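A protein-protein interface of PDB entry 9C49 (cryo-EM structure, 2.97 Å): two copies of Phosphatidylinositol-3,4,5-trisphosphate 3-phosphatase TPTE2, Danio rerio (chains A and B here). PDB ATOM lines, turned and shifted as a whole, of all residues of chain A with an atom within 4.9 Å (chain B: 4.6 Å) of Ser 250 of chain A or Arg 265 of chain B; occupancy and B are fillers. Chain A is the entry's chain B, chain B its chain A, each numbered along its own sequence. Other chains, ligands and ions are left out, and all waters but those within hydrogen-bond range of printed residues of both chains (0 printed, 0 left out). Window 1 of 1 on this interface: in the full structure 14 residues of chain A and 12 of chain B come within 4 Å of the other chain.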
ATOM      1  N   LEU A 248      29.276  18.208   7.800  1.00  0.00           N
ATOM      2  CA  LEU A 248      29.878  19.263   6.988  1.00  0.00           C
ATOM      3  C   LEU A 248      29.717  18.986   5.499  1.00  0.00           C
ATOM      4  O   LEU A 248      30.682  19.014   4.742  1.00  0.00           O
ATOM      5  CB  LEU A 248      31.347  19.422   7.351  1.00  0.00           C
ATOM      6  CG  LEU A 248      31.793  19.095   8.774  1.00  0.00           C
ATOM      7  CD1 LEU A 248      33.277  19.312   8.855  1.00  0.00           C
ATOM      8  CD2 LEU A 248      31.074  19.945   9.809  1.00  0.00           C
ATOM      9  N   CYS A 249      28.489  18.722   5.063  1.00  0.00           N
ATOM     10  CA  CYS A 249      28.196  18.458   3.660  1.00  0.00           C
ATOM     11  C   CYS A 249      27.145  19.444   3.184  1.00  0.00           C
ATOM     12  O   CYS A 249      26.061  19.527   3.767  1.00  0.00           O
ATOM     13  CB  CYS A 249      27.709  17.024   3.451  1.00  0.00           C
ATOM     14  SG  CYS A 249      28.973  15.772   3.669  1.00  0.00           S
ATOM     15  N   SER A 250      27.469  20.186   2.131  1.00  0.00           N
ATOM     16  CA  SER A 250      26.528  21.095   1.500  1.00  0.00           C
ATOM     17  C   SER A 250      25.762  20.439   0.364  1.00  0.00           C
ATOM     18  O   SER A 250      24.908  21.089  -0.247  1.00  0.00           O
ATOM     19  CB  SER A 250      27.265  22.330   0.979  1.00  0.00           C
ATOM     20  OG  SER A 250      26.432  23.112   0.145  1.00  0.00           O
ATOM     21  N   GLU A 251      26.040  19.169   0.072  1.00  0.00           N
ATOM     22  CA  GLU A 251      25.427  18.481  -1.050  1.00  0.00           C
ATOM     23  C   GLU A 251      24.557  17.300  -0.660  1.00  0.00           C
ATOM     24  O   GLU A 251      23.806  16.813  -1.511  1.00  0.00           O
ATOM     25  CB  GLU A 251      26.502  17.987  -2.030  1.00  0.00           C
ATOM     26  CG  GLU A 251      27.254  16.756  -1.554  1.00  0.00           C
ATOM     27  CD  GLU A 251      28.595  17.093  -0.932  1.00  0.00           C
ATOM     28  OE1 GLU A 251      28.746  18.210  -0.395  1.00  0.00           O
ATOM     29  OE2 GLU A 251      29.502  16.237  -0.986  1.00  0.00           O
ATOM     30  N   LYS A 252      24.633  16.820   0.578  1.00  0.00           N
ATOM     31  CA  LYS A 252      23.825  15.685   0.991  1.00  0.00           C
ATOM     32  C   LYS A 252      23.652  15.679   2.502  1.00  0.00           C
ATOM     33  O   LYS A 252      24.571  16.011   3.253  1.00  0.00           O
ATOM     34  CB  LYS A 252      24.450  14.365   0.523  1.00  0.00           C
ATOM     35  CG  LYS A 252      23.447  13.244   0.344  1.00  0.00           C
ATOM     36  CD  LYS A 252      23.939  11.959   0.971  1.00  0.00           C
ATOM     37  CE  LYS A 252      22.958  10.825   0.741  1.00  0.00           C
ATOM     38  NZ  LYS A 252      21.579  11.212   1.142  1.00  0.00           N
ATOM     39  N   ARG A 265      24.360  20.958  10.645  1.00  0.00           N
ATOM     40  CA  ARG A 265      24.892  20.909   9.293  1.00  0.00           C
ATOM     41  C   ARG A 265      25.670  22.189   9.029  1.00  0.00           C
ATOM     42  O   ARG A 265      25.146  23.291   9.226  1.00  0.00           O
ATOM     43  CB  ARG A 265      23.768  20.737   8.270  1.00  0.00           C
ATOM     44  CG  ARG A 265      23.144  19.348   8.251  1.00  0.00           C
ATOM     45  CD  ARG A 265      22.002  19.264   7.244  1.00  0.00           C
ATOM     46  NE  ARG A 265      22.407  18.644   5.987  1.00  0.00           N
ATOM     47  CZ  ARG A 265      22.729  19.314   4.888  1.00  0.00           C
ATOM     48  NH1 ARG A 265      22.702  20.634   4.852  1.00  0.00           N
ATOM     49  NH2 ARG A 265      23.087  18.641   3.799  1.00  0.00           N
ATOM     50  N   VAL A 266      26.917  22.041   8.597  1.00  0.00           N
ATOM     51  CA  VAL A 266      27.734  23.156   8.135  1.00  0.00           C
ATOM     52  C   VAL A 266      27.829  23.058   6.619  1.00  0.00           C
ATOM     53  O   VAL A 266      28.237  22.024   6.078  1.00  0.00           O
ATOM     54  CB  VAL A 266      29.124  23.143   8.788  1.00  0.00           C
ATOM     55  CG1 VAL A 266      29.902  24.385   8.403  1.00  0.00           C
ATOM     56  CG2 VAL A 266      28.991  23.046  10.299  1.00  0.00           C
ATOM     57  N   MET A 267      27.442  24.128   5.930  1.00  0.00           N
ATOM     58  CA  MET A 267      27.325  24.121   4.473  1.00  0.00           C
ATOM     59  C   MET A 267      28.689  24.400   3.864  1.00  0.00           C
ATOM     60  O   MET A 267      29.005  25.530   3.494  1.00  0.00           O
ATOM     61  CB  MET A 267      26.291  25.147   4.017  1.00  0.00           C
ATOM     62  CG  MET A 267      25.460  24.744   2.803  1.00  0.00           C
ATOM     63  SD  MET A 267      24.299  23.405   3.128  1.00  0.00           S
ATOM     64  CE  MET A 267      24.158  23.514   4.909  1.00  0.00           C
ATOM     65  N   ILE A 268      29.507  23.359   3.750  1.00  0.00           N
ATOM     66  CA  ILE A 268      30.813  23.453   3.108  1.00  0.00           C
ATOM     67  C   ILE A 268      30.766  22.642   1.825  1.00  0.00           C
ATOM     68  O   ILE A 268      30.427  21.453   1.850  1.00  0.00           O
ATOM     69  CB  ILE A 268      31.949  22.955   4.020  1.00  0.00           C
ATOM     70  CG1 ILE A 268      31.724  23.391   5.464  1.00  0.00           C
ATOM     71  CG2 ILE A 268      33.282  23.488   3.535  1.00  0.00           C
ATOM     72  CD1 ILE A 268      32.635  22.706   6.448  1.00  0.00           C
ATOM     73  N   ASP A 269      31.099  23.285   0.709  1.00  0.00           N
ATOM     74  CA  ASP A 269      31.168  22.603  -0.571  1.00  0.00           C
ATOM     75  C   ASP A 269      32.419  21.739  -0.644  1.00  0.00           C
ATOM     76  O   ASP A 269      33.440  22.034  -0.018  1.00  0.00           O
ATOM     77  CB  ASP A 269      31.167  23.613  -1.717  1.00  0.00           C
ATOM     78  CG  ASP A 269      29.812  24.255  -1.926  1.00  0.00           C
ATOM     79  OD1 ASP A 269      28.972  24.192  -1.006  1.00  0.00           O
ATOM     80  OD2 ASP A 269      29.585  24.821  -3.016  1.00  0.00           O
ATOM     81  N   ARG A 308      37.186  18.609   4.247  1.00  0.00           N
ATOM     82  CA  ARG A 308      36.332  19.472   5.052  1.00  0.00           C
ATOM     83  C   ARG A 308      36.323  19.044   6.513  1.00  0.00           C
ATOM     84  O   ARG A 308      36.413  19.886   7.414  1.00  0.00           O
ATOM     85  CB  ARG A 308      34.919  19.474   4.477  1.00  0.00           C
ATOM     86  CG  ARG A 308      34.834  20.098   3.104  1.00  0.00           C
ATOM     87  CD  ARG A 308      33.439  19.983   2.546  1.00  0.00           C
ATOM     88  NE  ARG A 308      33.101  18.599   2.246  1.00  0.00           N
ATOM     89  CZ  ARG A 308      31.986  18.216   1.645  1.00  0.00           C
ATOM     90  NH1 ARG A 308      31.077  19.093   1.253  1.00  0.00           N
ATOM     91  NH2 ARG A 308      31.778  16.923   1.425  1.00  0.00           N
ATOM     92  N   ASN B 247      16.045  24.771  -4.913  1.00  0.00           N
ATOM     93  CA  ASN B 247      16.268  23.386  -4.512  1.00  0.00           C
ATOM     94  C   ASN B 247      15.747  23.228  -3.091  1.00  0.00           C
ATOM     95  O   ASN B 247      16.487  23.418  -2.123  1.00  0.00           O
ATOM     96  CB  ASN B 247      17.746  23.029  -4.621  1.00  0.00           C
ATOM     97  CG  ASN B 247      18.059  21.660  -4.059  1.00  0.00           C
ATOM     98  OD1 ASN B 247      18.953  21.509  -3.232  1.00  0.00           O
ATOM     99  ND2 ASN B 247      17.317  20.657  -4.498  1.00  0.00           N
ATOM    100  N   CYS B 249      15.404  21.015  -0.973  1.00  0.00           N
ATOM    101  CA  CYS B 249      15.803  19.726  -0.429  1.00  0.00           C
ATOM    102  C   CYS B 249      16.757  19.955   0.729  1.00  0.00           C
ATOM    103  O   CYS B 249      17.800  20.595   0.561  1.00  0.00           O
ATOM    104  CB  CYS B 249      16.455  18.848  -1.498  1.00  0.00           C
ATOM    105  SG  CYS B 249      15.339  18.320  -2.796  1.00  0.00           S
ATOM    106  N   LYS B 252      19.508  16.687  -0.261  1.00  0.00           N
ATOM    107  CA  LYS B 252      20.252  16.492  -1.496  1.00  0.00           C
ATOM    108  C   LYS B 252      20.508  17.832  -2.165  1.00  0.00           C
ATOM    109  O   LYS B 252      19.639  18.707  -2.200  1.00  0.00           O
ATOM    110  CB  LYS B 252      19.504  15.559  -2.456  1.00  0.00           C
ATOM    111  CG  LYS B 252      20.393  14.816  -3.440  1.00  0.00           C
ATOM    112  CD  LYS B 252      20.958  13.539  -2.844  1.00  0.00           C
ATOM    113  CE  LYS B 252      22.258  13.142  -3.531  1.00  0.00           C
ATOM    114  NZ  LYS B 252      23.072  12.202  -2.711  1.00  0.00           N
ATOM    115  N   GLY B 253      21.719  17.986  -2.688  1.00  0.00           N
ATOM    116  CA  GLY B 253      22.076  19.152  -3.471  1.00  0.00           C
ATOM    117  C   GLY B 253      23.174  18.779  -4.435  1.00  0.00           C
ATOM    118  O   GLY B 253      23.932  17.837  -4.192  1.00  0.00           O
ATOM    119  N   VAL B 263      21.012  29.382  -7.752  1.00  0.00           N
ATOM    120  CA  VAL B 263      20.383  28.266  -7.055  1.00  0.00           C
ATOM    121  C   VAL B 263      20.243  28.631  -5.586  1.00  0.00           C
ATOM    122  O   VAL B 263      21.239  28.943  -4.922  1.00  0.00           O
ATOM    123  CB  VAL B 263      21.197  26.967  -7.212  1.00  0.00           C
ATOM    124  CG1 VAL B 263      20.766  25.947  -6.178  1.00  0.00           C
ATOM    125  CG2 VAL B 263      21.056  26.391  -8.603  1.00  0.00           C
ATOM    126  N   GLU B 264      19.021  28.600  -5.061  1.00  0.00           N
ATOM    127  CA  GLU B 264      18.791  28.804  -3.639  1.00  0.00           C
ATOM    128  C   GLU B 264      18.193  27.556  -3.014  1.00  0.00           C
ATOM    129  O   GLU B 264      17.216  26.998  -3.524  1.00  0.00           O
ATOM    130  CB  GLU B 264      17.881  29.999  -3.372  1.00  0.00           C
ATOM    131  CG  GLU B 264      18.043  31.122  -4.358  1.00  0.00           C
ATOM    132  CD  GLU B 264      18.021  32.473  -3.676  1.00  0.00           C
ATOM    133  OE1 GLU B 264      17.514  32.551  -2.537  1.00  0.00           O
ATOM    134  OE2 GLU B 264      18.527  33.452  -4.260  1.00  0.00           O
ATOM    135  N   ARG B 265      18.781  27.135  -1.902  1.00  0.00           N
ATOM    136  CA  ARG B 265      18.378  25.932  -1.189  1.00  0.00           C
ATOM    137  C   ARG B 265      17.500  26.330  -0.013  1.00  0.00           C
ATOM    138  O   ARG B 265      17.910  27.139   0.825  1.00  0.00           O
ATOM    139  CB  ARG B 265      19.599  25.159  -0.696  1.00  0.00           C
ATOM    140  CG  ARG B 265      20.472  24.576  -1.787  1.00  0.00           C
ATOM    141  CD  ARG B 265      21.616  23.788  -1.173  1.00  0.00           C
ATOM    142  NE  ARG B 265      21.396  22.350  -1.233  1.00  0.00           N
ATOM    143  CZ  ARG B 265      20.790  21.642  -0.291  1.00  0.00           C
ATOM    144  NH1 ARG B 265      20.279  22.216   0.782  1.00  0.00           N
ATOM    145  NH2 ARG B 265      20.687  20.326  -0.433  1.00  0.00           N
ATOM    146  N   VAL B 266      16.301  25.765   0.046  1.00  0.00           N
ATOM    147  CA  VAL B 266      15.408  25.921   1.186  1.00  0.00           C
ATOM    148  C   VAL B 266      15.393  24.599   1.939  1.00  0.00           C
ATOM    149  O   VAL B 266      15.037  23.559   1.376  1.00  0.00           O
ATOM    150  CB  VAL B 266      13.997  26.330   0.742  1.00  0.00           C
ATOM    151  CG1 VAL B 266      13.151  26.690   1.945  1.00  0.00           C
ATOM    152  CG2 VAL B 266      14.073  27.498  -0.219  1.00  0.00           C
ATOM    153  N   MET B 267      15.783  24.634   3.211  1.00  0.00           N
ATOM    154  CA  MET B 267      15.949  23.417   4.003  1.00  0.00           C
ATOM    155  C   MET B 267      14.570  22.918   4.403  1.00  0.00           C
ATOM    156  O   MET B 267      14.066  23.223   5.484  1.00  0.00           O
ATOM    157  CB  MET B 267      16.806  23.678   5.234  1.00  0.00           C
ATOM    158  CG  MET B 267      18.249  24.059   4.968  1.00  0.00           C
ATOM    159  SD  MET B 267      19.102  23.097   3.712  1.00  0.00           S
ATOM    160  CE  MET B 267      20.108  24.395   3.002  1.00  0.00           C
ATOM    161  N   ARG B 281      11.265  34.380   3.506  1.00  0.00           N
ATOM    162  CA  ARG B 281      12.481  34.620   2.732  1.00  0.00           C
ATOM    163  C   ARG B 281      12.342  34.091   1.311  1.00  0.00           C
ATOM    164  O   ARG B 281      12.820  34.714   0.355  1.00  0.00           O
ATOM    165  CB  ARG B 281      13.681  33.976   3.423  1.00  0.00           C
ATOM    166  CG  ARG B 281      15.022  34.454   2.895  1.00  0.00           C
ATOM    167  CD  ARG B 281      16.173  33.641   3.467  1.00  0.00           C
ATOM    168  NE  ARG B 281      16.286  32.323   2.854  1.00  0.00           N
ATOM    169  CZ  ARG B 281      15.874  31.196   3.418  1.00  0.00           C
ATOM    170  NH1 ARG B 281      15.290  31.190   4.606  1.00  0.00           N
ATOM    171  NH2 ARG B 281      16.055  30.045   2.777  1.00  0.00           N
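The backbone NH (N) of Gly 253 of chain B is in hydrogen-bond range of the backbone carbonyl oxygen (O) of Glu 251 of chain A.
OD1 of Asn 247 of chain B is in hydrogen-bond range of NE of Arg 265 of chain B (3.3 Å). The backbone carbonyl oxygen (O) of Ile 268 of chain A lies within hydrogen-bond range of the backbone NH (N) of Ser 250 of chain A (3.2 Å). SD of Met 267 of chain A lies close to OG of Ser 250 of chain A. NH1 of Arg 265 of chain B lies close to SD of Met 267 of chain B (3.3 Å). O of Lys 252 of chain A lies within hydrogen-bond range of NH2 of Arg 265 of chain A, 3.1 Å away. The side-chain amide oxygen (OD1) of Asn 247 of chain B sits close to the backbone carbonyl oxygen (O) of Lys 252 of chain B, 3.1 Å away.
Arg 265 of chain B touches Ser 250 of chain A. Glu 251 of chain A touches Lys 252 of chain B (O to C, 3.5 Å). Lys 252 of chain A touches Lys 252 of chain B (CG to NZ, 3.2 Å).
Arg 265 of chain B touches one residue of chain A. Of the printed residues of chain A, Lys 252 of chain B touches Glu 251 and Lys 252. Of the printed residues of chain A, Gly 253 of chain B touches Glu 251. Printed residues of chain B within 4 Å of Glu 251 of chain A: Lys 252 (3.5 Å) and Gly 253 (2.7 Å). Asp 269 of chain A touches none of the printed residues of chain B. Met 267 of chain A touches none of the printed residues of chain B. The nearest printed residue of chain B that does not touch Ser 250 of chain A is Gly 253 of chain B (4.7 Å). The nearest printed residue of chain B that does not touch Lys 252 of chain A is Gly 253 of chain B (4.5 Å).
Printed residues of chain A that touch a printed residue of chain B: Ser 250, Glu 251 and Lys 252. Among the printed residues, 4 pairs touch across the chains. Among the printed residues, no Asp or Glu carboxylate lies within 4 Å of a Lys or Arg side-chain nitrogen of the other chain.
Lys 252 of chain B touches its own counterpart, Lys 252 of chain A. 5 positions are printed for both chains. Of the 4 pairs that touch across the chains among the printed residues, 1 has its exchanged pair printed and touching as well.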
